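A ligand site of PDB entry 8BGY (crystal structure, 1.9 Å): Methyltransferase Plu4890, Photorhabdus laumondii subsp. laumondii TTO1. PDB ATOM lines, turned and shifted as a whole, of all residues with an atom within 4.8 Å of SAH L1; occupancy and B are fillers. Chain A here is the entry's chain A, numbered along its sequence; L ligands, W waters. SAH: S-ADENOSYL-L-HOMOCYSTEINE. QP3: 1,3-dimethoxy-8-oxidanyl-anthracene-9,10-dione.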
ATOM      1  N   PHE A 127      19.283 -16.452  -1.112  1.00  0.00           N
ATOM      2  CA  PHE A 127      18.781 -17.104  -2.352  1.00  0.00           C
ATOM      3  C   PHE A 127      19.947 -17.701  -3.160  1.00  0.00           C
ATOM      4  O   PHE A 127      19.761 -18.788  -3.742  1.00  0.00           O
ATOM      5  CB  PHE A 127      17.944 -16.119  -3.170  1.00  0.00           C
ATOM      6  CG  PHE A 127      16.601 -15.828  -2.563  1.00  0.00           C
ATOM      7  CD1 PHE A 127      15.672 -16.849  -2.364  1.00  0.00           C
ATOM      8  CD2 PHE A 127      16.247 -14.543  -2.175  1.00  0.00           C
ATOM      9  CE1 PHE A 127      14.438 -16.592  -1.796  1.00  0.00           C
ATOM     10  CE2 PHE A 127      15.010 -14.281  -1.615  1.00  0.00           C
ATOM     11  CZ  PHE A 127      14.107 -15.312  -1.429  1.00  0.00           C
ATOM     12  N   PHE A 140      11.936 -24.445   1.503  1.00  0.00           N
ATOM     13  CA  PHE A 140      11.539 -23.014   1.359  1.00  0.00           C
ATOM     14  C   PHE A 140      10.540 -22.873   0.205  1.00  0.00           C
ATOM     15  O   PHE A 140       9.469 -22.265   0.413  1.00  0.00           O
ATOM     16  CB  PHE A 140      12.752 -22.107   1.134  1.00  0.00           C
ATOM     17  CG  PHE A 140      12.388 -20.654   0.922  1.00  0.00           C
ATOM     18  CD1 PHE A 140      12.162 -19.820   2.002  1.00  0.00           C
ATOM     19  CD2 PHE A 140      12.240 -20.145  -0.357  1.00  0.00           C
ATOM     20  CE1 PHE A 140      11.809 -18.492   1.812  1.00  0.00           C
ATOM     21  CE2 PHE A 140      11.888 -18.817  -0.547  1.00  0.00           C
ATOM     22  CZ  PHE A 140      11.672 -17.991   0.538  1.00  0.00           C
ATOM     23  N   MET A 144       6.543 -21.662   0.365  1.00  0.00           N
ATOM     24  CA  MET A 144       6.025 -20.569  -0.508  1.00  0.00           C
ATOM     25  C   MET A 144       4.851 -21.096  -1.345  1.00  0.00           C
ATOM     26  O   MET A 144       3.869 -20.355  -1.513  1.00  0.00           O
ATOM     27  CB  MET A 144       7.106 -20.027  -1.440  1.00  0.00           C
ATOM     28  CG  MET A 144       8.269 -19.338  -0.723  1.00  0.00           C
ATOM     29  SD  MET A 144       7.746 -18.037   0.430  1.00  0.00           S
ATOM     30  CE  MET A 144       7.687 -18.965   1.961  1.00  0.00           C
ATOM     31  N   THR A 145       4.963 -22.329  -1.858  1.00  0.00           N
ATOM     32  CA  THR A 145       3.921 -23.014  -2.667  1.00  0.00           C
ATOM     33  C   THR A 145       2.643 -23.203  -1.826  1.00  0.00           C
ATOM     34  O   THR A 145       1.549 -22.934  -2.364  1.00  0.00           O
ATOM     35  CB  THR A 145       4.448 -24.348  -3.214  1.00  0.00           C
ATOM     36  OG1 THR A 145       5.366 -24.033  -4.259  1.00  0.00           O
ATOM     37  CG2 THR A 145       3.363 -25.261  -3.748  1.00  0.00           C
ATOM     38  N   VAL A 147       1.590 -21.573   1.052  1.00  0.00           N
ATOM     39  CA  VAL A 147       0.972 -20.255   1.427  1.00  0.00           C
ATOM     40  C   VAL A 147       0.363 -19.608   0.182  1.00  0.00           C
ATOM     41  O   VAL A 147      -0.687 -18.947   0.319  1.00  0.00           O
ATOM     42  CB  VAL A 147       1.975 -19.313   2.130  1.00  0.00           C
ATOM     43  CG1 VAL A 147       2.435 -19.888   3.471  1.00  0.00           C
ATOM     44  CG2 VAL A 147       3.172 -18.958   1.263  1.00  0.00           C
ATOM     45  N   SER A 148       0.989 -19.782  -0.991  1.00  0.00           N
ATOM     46  CA  SER A 148       0.450 -19.329  -2.305  1.00  0.00           C
ATOM     47  C   SER A 148      -0.895 -20.010  -2.565  1.00  0.00           C
ATOM     48  O   SER A 148      -1.828 -19.309  -2.981  1.00  0.00           O
ATOM     49  CB  SER A 148       1.427 -19.600  -3.432  1.00  0.00           C
ATOM     50  OG  SER A 148       2.581 -18.785  -3.302  1.00  0.00           O
ATOM     51  N   VAL A 170       6.124 -12.281 -11.146  1.00  0.00           N
ATOM     52  CA  VAL A 170       7.566 -11.983 -10.949  1.00  0.00           C
ATOM     53  C   VAL A 170       7.989 -12.496  -9.563  1.00  0.00           C
ATOM     54  O   VAL A 170       7.335 -12.126  -8.570  1.00  0.00           O
ATOM     55  CB  VAL A 170       7.860 -10.475 -11.108  1.00  0.00           C
ATOM     56  CG1 VAL A 170       9.314 -10.139 -10.869  1.00  0.00           C
ATOM     57  CG2 VAL A 170       7.410  -9.966 -12.476  1.00  0.00           C
ATOM     58  N   GLY A 171       9.051 -13.307  -9.516  1.00  0.00           N
ATOM     59  CA  GLY A 171       9.486 -14.044  -8.317  1.00  0.00           C
ATOM     60  C   GLY A 171       8.415 -15.017  -7.850  1.00  0.00           C
ATOM     61  O   GLY A 171       8.149 -15.059  -6.642  1.00  0.00           O
ATOM     62  N   GLY A 172       7.823 -15.771  -8.791  1.00  0.00           N
ATOM     63  CA  GLY A 172       6.669 -16.654  -8.558  1.00  0.00           C
ATOM     64  C   GLY A 172       7.064 -18.022  -8.014  1.00  0.00           C
ATOM     65  O   GLY A 172       6.145 -18.816  -7.728  1.00  0.00           O
ATOM     66  N   GLY A 173       8.371 -18.291  -7.879  1.00  0.00           N
ATOM     67  CA  GLY A 173       8.905 -19.548  -7.325  1.00  0.00           C
ATOM     68  C   GLY A 173       8.591 -20.736  -8.210  1.00  0.00           C
ATOM     69  O   GLY A 173       8.982 -20.699  -9.398  1.00  0.00           O
ATOM     70  N   LEU A 193       8.254 -15.639 -13.733  1.00  0.00           N
ATOM     71  CA  LEU A 193       9.692 -15.250 -13.732  1.00  0.00           C
ATOM     72  C   LEU A 193      10.279 -15.518 -12.340  1.00  0.00           C
ATOM     73  O   LEU A 193       9.659 -15.097 -11.340  1.00  0.00           O
ATOM     74  CB  LEU A 193       9.817 -13.779 -14.110  1.00  0.00           C
ATOM     75  CG  LEU A 193      11.247 -13.279 -14.352  1.00  0.00           C
ATOM     76  CD1 LEU A 193      11.280 -12.167 -15.385  1.00  0.00           C
ATOM     77  CD2 LEU A 193      11.903 -12.819 -13.061  1.00  0.00           C
ATOM     78  N   ASP A 194      11.439 -16.191 -12.293  1.00  0.00           N
ATOM     79  CA  ASP A 194      12.232 -16.451 -11.062  1.00  0.00           C
ATOM     80  C   ASP A 194      13.651 -16.844 -11.488  1.00  0.00           C
ATOM     81  O   ASP A 194      13.949 -16.746 -12.698  1.00  0.00           O
ATOM     82  CB  ASP A 194      11.560 -17.514 -10.195  1.00  0.00           C
ATOM     83  CG  ASP A 194      11.825 -17.360  -8.702  1.00  0.00           C
ATOM     84  OD1 ASP A 194      12.994 -17.497  -8.302  1.00  0.00           O
ATOM     85  OD2 ASP A 194      10.858 -17.093  -7.957  1.00  0.00           O
ATOM     86  N   ARG A 195      14.500 -17.243 -10.539  1.00  0.00           N
ATOM     87  CA  ARG A 195      15.881 -17.720 -10.788  1.00  0.00           C
ATOM     88  C   ARG A 195      15.868 -19.242 -10.907  1.00  0.00           C
ATOM     89  O   ARG A 195      15.784 -19.926  -9.870  1.00  0.00           O
ATOM     90  CB  ARG A 195      16.820 -17.241  -9.675  1.00  0.00           C
ATOM     91  CG  ARG A 195      16.903 -15.722  -9.555  1.00  0.00           C
ATOM     92  CD  ARG A 195      17.763 -15.264  -8.395  1.00  0.00           C
ATOM     93  NE  ARG A 195      19.150 -15.693  -8.525  1.00  0.00           N
ATOM     94  CZ  ARG A 195      19.690 -16.760  -7.939  1.00  0.00           C
ATOM     95  NH1 ARG A 195      18.971 -17.542  -7.162  1.00  0.00           N
ATOM     96  NH2 ARG A 195      20.962 -17.046  -8.145  1.00  0.00           N
ATOM     97  N   GLY A 210      14.981 -15.186 -15.115  1.00  0.00           N
ATOM     98  CA  GLY A 210      15.238 -13.735 -15.164  1.00  0.00           C
ATOM     99  C   GLY A 210      15.797 -13.199 -13.863  1.00  0.00           C
ATOM    100  O   GLY A 210      16.107 -14.005 -12.960  1.00  0.00           O
ATOM    101  N   ASN A 211      15.943 -11.870 -13.783  1.00  0.00           N
ATOM    102  CA  ASN A 211      16.456 -11.125 -12.612  1.00  0.00           C
ATOM    103  C   ASN A 211      15.724  -9.785 -12.533  1.00  0.00           C
ATOM    104  O   ASN A 211      16.003  -8.919 -13.384  1.00  0.00           O
ATOM    105  CB  ASN A 211      17.983 -10.943 -12.705  1.00  0.00           C
ATOM    106  CG  ASN A 211      18.593 -10.300 -11.476  1.00  0.00           C
ATOM    107  OD1 ASN A 211      17.907 -10.025 -10.502  1.00  0.00           O
ATOM    108  ND2 ASN A 211      19.893 -10.055 -11.528  1.00  0.00           N
ATOM    109  N   PHE A 212      14.817  -9.628 -11.560  1.00  0.00           N
ATOM    110  CA  PHE A 212      13.925  -8.434 -11.433  1.00  0.00           C
ATOM    111  C   PHE A 212      14.724  -7.209 -10.975  1.00  0.00           C
ATOM    112  O   PHE A 212      14.177  -6.087 -11.069  1.00  0.00           O
ATOM    113  CB  PHE A 212      12.718  -8.715 -10.522  1.00  0.00           C
ATOM    114  CG  PHE A 212      12.985  -9.341  -9.177  1.00  0.00           C
ATOM    115  CD1 PHE A 212      12.290 -10.475  -8.779  1.00  0.00           C
ATOM    116  CD2 PHE A 212      13.881  -8.776  -8.287  1.00  0.00           C
ATOM    117  CE1 PHE A 212      12.507 -11.034  -7.536  1.00  0.00           C
ATOM    118  CE2 PHE A 212      14.110  -9.342  -7.040  1.00  0.00           C
ATOM    119  CZ  PHE A 212      13.414 -10.478  -6.665  1.00  0.00           C
ATOM    120  N   LEU A 213      15.963  -7.395 -10.516  1.00  0.00           N
ATOM    121  CA  LEU A 213      16.906  -6.289 -10.176  1.00  0.00           C
ATOM    122  C   LEU A 213      17.422  -5.632 -11.459  1.00  0.00           C
ATOM    123  O   LEU A 213      17.710  -4.424 -11.428  1.00  0.00           O
ATOM    124  CB  LEU A 213      18.076  -6.838  -9.344  1.00  0.00           C
ATOM    125  CG  LEU A 213      17.711  -7.418  -7.980  1.00  0.00           C
ATOM    126  CD1 LEU A 213      18.944  -8.022  -7.314  1.00  0.00           C
ATOM    127  CD2 LEU A 213      17.090  -6.365  -7.078  1.00  0.00           C
ATOM    128  N   LYS A 226       4.301 -10.961  -5.331  1.00  0.00           N
ATOM    129  CA  LYS A 226       3.730 -11.505  -4.077  1.00  0.00           C
ATOM    130  C   LYS A 226       4.861 -11.950  -3.140  1.00  0.00           C
ATOM    131  O   LYS A 226       5.639 -12.840  -3.538  1.00  0.00           O
ATOM    132  CB  LYS A 226       2.781 -12.667  -4.386  1.00  0.00           C
ATOM    133  CG  LYS A 226       1.975 -13.183  -3.202  1.00  0.00           C
ATOM    134  CD  LYS A 226       0.974 -14.265  -3.582  1.00  0.00           C
ATOM    135  CE  LYS A 226       0.851 -15.362  -2.550  1.00  0.00           C
ATOM    136  NZ  LYS A 226       2.078 -16.181  -2.473  1.00  0.00           N
ATOM    137  N   ASN A 227       4.937 -11.344  -1.944  1.00  0.00           N
ATOM    138  CA  ASN A 227       5.914 -11.679  -0.879  1.00  0.00           C
ATOM    139  C   ASN A 227       7.334 -11.689  -1.447  1.00  0.00           C
ATOM    140  O   ASN A 227       8.017 -12.725  -1.332  1.00  0.00           O
ATOM    141  CB  ASN A 227       5.576 -13.015  -0.200  1.00  0.00           C
ATOM    142  CG  ASN A 227       4.325 -12.976   0.642  1.00  0.00           C
ATOM    143  OD1 ASN A 227       3.886 -11.914   1.072  1.00  0.00           O
ATOM    144  ND2 ASN A 227       3.735 -14.135   0.890  1.00  0.00           N
ATOM    145  N   VAL A 228       7.757 -10.584  -2.065  1.00  0.00           N
ATOM    146  CA  VAL A 228       9.130 -10.388  -2.624  1.00  0.00           C
ATOM    147  C   VAL A 228       9.822  -9.241  -1.871  1.00  0.00           C
ATOM    148  O   VAL A 228      10.956  -9.449  -1.394  1.00  0.00           O
ATOM    149  CB  VAL A 228       9.101 -10.134  -4.136  1.00  0.00           C
ATOM    150  CG1 VAL A 228      10.442  -9.638  -4.673  1.00  0.00           C
ATOM    151  CG2 VAL A 228       8.646 -11.370  -4.912  1.00  0.00           C
ATOM    152  N   ASN A 231      12.139  -9.089   1.257  1.00  0.00           N
ATOM    153  CA  ASN A 231      13.482  -9.714   1.137  1.00  0.00           C
ATOM    154  C   ASN A 231      14.509  -8.665   0.690  1.00  0.00           C
ATOM    155  O   ASN A 231      15.691  -9.039   0.531  1.00  0.00           O
ATOM    156  CB  ASN A 231      13.498 -10.874   0.138  1.00  0.00           C
ATOM    157  CG  ASN A 231      12.463 -11.938   0.414  1.00  0.00           C
ATOM    158  OD1 ASN A 231      11.965 -12.580  -0.516  1.00  0.00           O
ATOM    159  ND2 ASN A 231      12.135 -12.162   1.681  1.00  0.00           N
ATOM    160  N   TRP A 232      14.100  -7.410   0.488  1.00  0.00           N
ATOM    161  CA  TRP A 232      14.927  -6.345  -0.140  1.00  0.00           C
ATOM    162  C   TRP A 232      14.875  -5.050   0.685  1.00  0.00           C
ATOM    163  O   TRP A 232      13.835  -4.793   1.315  1.00  0.00           O
ATOM    164  CB  TRP A 232      14.496  -6.120  -1.588  1.00  0.00           C
ATOM    165  CG  TRP A 232      14.565  -7.365  -2.414  1.00  0.00           C
ATOM    166  CD1 TRP A 232      13.533  -8.184  -2.769  1.00  0.00           C
ATOM    167  CD2 TRP A 232      15.758  -7.977  -2.943  1.00  0.00           C
ATOM    168  NE1 TRP A 232      13.993  -9.239  -3.496  1.00  0.00           N
ATOM    169  CE2 TRP A 232      15.352  -9.144  -3.624  1.00  0.00           C
ATOM    170  CE3 TRP A 232      17.121  -7.648  -2.930  1.00  0.00           C
ATOM    171  CZ2 TRP A 232      16.260  -9.969  -4.282  1.00  0.00           C
ATOM    172  CZ3 TRP A 232      18.014  -8.472  -3.572  1.00  0.00           C
ATOM    173  CH2 TRP A 232      17.588  -9.621  -4.237  1.00  0.00           C
HETATM  174  N   SAH L   1       6.061 -15.066  -5.031  1.00  0.00           N
HETATM  175  CA  SAH L   1       6.204 -16.415  -4.392  1.00  0.00           C
HETATM  176  CB  SAH L   1       7.614 -16.635  -3.847  1.00  0.00           C
HETATM  177  CG  SAH L   1       8.063 -15.561  -2.865  1.00  0.00           C
HETATM  178  SD  SAH L   1       9.687 -15.909  -2.147  1.00  0.00           S
HETATM  179  C   SAH L   1       5.187 -16.551  -3.255  1.00  0.00           C
HETATM  180  O   SAH L   1       4.909 -17.647  -2.779  1.00  0.00           O
HETATM  181  OXT SAH L   1       4.619 -15.562  -2.792  1.00  0.00           O
HETATM  182  C5' SAH L   1      10.761 -14.800  -3.093  1.00  0.00           C
HETATM  183  C4' SAH L   1      11.073 -15.323  -4.473  1.00  0.00           C
HETATM  184  O4' SAH L   1      11.905 -14.367  -5.174  1.00  0.00           O
HETATM  185  C3' SAH L   1      11.831 -16.662  -4.500  1.00  0.00           C
HETATM  186  O3' SAH L   1      11.157 -17.596  -5.329  1.00  0.00           O
HETATM  187  C2' SAH L   1      13.201 -16.288  -5.078  1.00  0.00           C
HETATM  188  O2' SAH L   1      13.782 -17.328  -5.832  1.00  0.00           O
HETATM  189  C1' SAH L   1      12.840 -15.090  -5.949  1.00  0.00           C
HETATM  190  N9  SAH L   1      13.960 -14.214  -6.271  1.00  0.00           N
HETATM  191  C8  SAH L   1      14.936 -13.763  -5.419  1.00  0.00           C
HETATM  192  N7  SAH L   1      15.813 -12.979  -5.993  1.00  0.00           N
HETATM  193  C5  SAH L   1      15.381 -12.901  -7.310  1.00  0.00           C
HETATM  194  C6  SAH L   1      15.891 -12.217  -8.434  1.00  0.00           C
HETATM  195  N6  SAH L   1      16.979 -11.447  -8.405  1.00  0.00           N
HETATM  196  N1  SAH L   1      15.218 -12.353  -9.600  1.00  0.00           N
HETATM  197  C2  SAH L   1      14.126 -13.130  -9.632  1.00  0.00           C
HETATM  198  N3  SAH L   1      13.559 -13.814  -8.645  1.00  0.00           N
HETATM  199  C4  SAH L   1      14.241 -13.664  -7.497  1.00  0.00           C
HETATM  200  CAU QP3 L   2      12.289 -17.206   5.625  1.00  0.00           C
HETATM  201  OAT QP3 L   2      10.892 -17.092   5.925  1.00  0.00           O
HETATM  202  CAL QP3 L   2      10.087 -16.507   4.996  1.00  0.00           C
HETATM  203  CAK QP3 L   2      10.570 -15.716   3.950  1.00  0.00           C
HETATM  204  CAM QP3 L   2       8.703 -16.735   5.127  1.00  0.00           C
HETATM  205  CAN QP3 L   2       8.212 -17.522   6.177  1.00  0.00           C
HETATM  206  OAO QP3 L   2       8.974 -18.039   6.991  1.00  0.00           O
HETATM  207  CAP QP3 L   2       6.836 -17.736   6.290  1.00  0.00           C
HETATM  208  CAQ QP3 L   2       6.319 -18.515   7.329  1.00  0.00           C
HETATM  209  OAR QP3 L   2       7.203 -19.062   8.197  1.00  0.00           O
HETATM  210  CAS QP3 L   2       4.957 -18.742   7.455  1.00  0.00           C
HETATM  211  CAA QP3 L   2       4.082 -18.170   6.538  1.00  0.00           C
HETATM  212  CAB QP3 L   2       4.580 -17.379   5.500  1.00  0.00           C
HETATM  213  CAC QP3 L   2       5.951 -17.156   5.369  1.00  0.00           C
HETATM  214  CAD QP3 L   2       6.445 -16.374   4.328  1.00  0.00           C
HETATM  215  OAE QP3 L   2       5.665 -15.870   3.511  1.00  0.00           O
HETATM  216  CAF QP3 L   2       7.820 -16.160   4.215  1.00  0.00           C
HETATM  217  CAG QP3 L   2       8.316 -15.365   3.168  1.00  0.00           C
HETATM  218  CAH QP3 L   2       9.693 -15.157   3.039  1.00  0.00           C
HETATM  219  OAI QP3 L   2      10.248 -14.384   2.057  1.00  0.00           O
HETATM  220  CAJ QP3 L   2       9.704 -14.412   0.737  1.00  0.00           C
HETATM  221  O   HOH W   1       5.247 -12.953  -7.034  1.00  0.00           O
HETATM  222  O   HOH W   2       9.885 -19.950  -3.918  1.00  0.00           O
HETATM  223  O   HOH W   3       3.571 -15.954  -6.336  1.00  0.00           O
HETATM  224  O   HOH W   4      12.677 -12.252  -3.321  1.00  0.00           O
HETATM  225  O   HOH W   5      18.792 -13.022  -5.403  1.00  0.00           O
HETATM  226  O   HOH W   6      16.389 -17.837  -6.122  1.00  0.00           O
HETATM  227  O   HOH W   7       5.437 -19.741  -4.394  1.00  0.00           O
HETATM  228  O   HOH W   8       4.960 -16.553   0.002  1.00  0.00           O
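The side-chain carboxylate (OD1) of Asp 194 lies within hydrogen-bond range of an oxygen (O2') of SAH L1 (2.6 Å).
O of Lys 226 sits at hydrogen-bond distance from N of SAH L1 (2.7 Å).
The side-chain amino group (NZ) of Lys 226 is in salt-bridge range of an oxygen (OXT) of SAH L1 (2.6 Å).
N of SAH L1 is in hydrogen-bond range of O of Gly 171 (2.6 Å).
The side-chain hydroxyl of Ser 148 lies within hydrogen-bond range of an oxygen (O) of SAH L1 (2.6 Å).
A nitrogen (N6) of SAH L1 sits at hydrogen-bond distance from the side-chain amide oxygen of Asn 211, 2.7 Å away.
N of Phe 212 lies within hydrogen-bond range of N1 of SAH L1, at 3.4 Å.
ND2 of Asn 231 is in hydrogen-bond range of OAI of QP3 L2 (2.9 Å).
N of Gly 210 is in hydrogen-bond range of O of Asp 194, 3.1 Å away.
OD2 of Asp 194 lies within hydrogen-bond range of N of Gly 172, at 3.4 Å.
The side-chain amino group (NZ) of Lys 226 lies within hydrogen-bond range of the side-chain hydroxyl (OG) of Ser 148 (2.8 Å).
O of Leu 193 is in hydrogen-bond range of N of Gly 171 (2.6 Å).
OG of Ser 148 is in hydrogen-bond range of O of Met 144, 2.7 Å away.
OD1 of Asn 211 sits close to N of Leu 213, 3.3 Å away.
The side-chain amide oxygen of Asn 231 sits close to the backbone carbonyl oxygen of Val 228 (3.4 Å).
The backbone carbonyl oxygen (O) of Leu 193 is in hydrogen-bond range of the backbone NH (N) of Gly 172 (3.2 Å).
The backbone carbonyl oxygen (O) of Met 144 lies close to an oxygen (O) of SAH L1 (3.2 Å).
SD of SAH L1 lies close to O of Asn 227 (3.7 Å).
Residues that only touch SAH L1: Trp 232, Phe 127, Arg 195, Gly 173, Asn 231, Gly 210, Gly 172 and Phe 140.
Of the 22 residues printed, 16 come within 4 Å of SAH L1.
Water W6 lies within hydrogen-bond range of an oxygen (O2') of SAH L1 and the guanidinium group of Arg 195.
Water W7 lies within hydrogen-bond range of an oxygen (O) of SAH L1 (2.7 Å), the side-chain hydroxyl of Ser 148 (3.2 Å) and the backbone carbonyl oxygen of Met 144 (3.3 Å).
Water W4 lies within hydrogen-bond range of the side-chain amide oxygen (OD1) of Asn 231, an oxygen (O4') of SAH L1 and the indole nitrogen (NE1) of Trp 232.
Water W8 lies within hydrogen-bond range of ND2 of Asn 227 (2.9 Å), OXT of SAH L1 (3.0 Å) and SD of Met 144 (3.2 Å).
Water W1 lies within hydrogen-bond range of the backbone carbonyl oxygen (O) of Val 170 (2.7 Å), the backbone NH (N) of Lys 226 (2.8 Å) and a nitrogen (N) of SAH L1 (3.0 Å).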
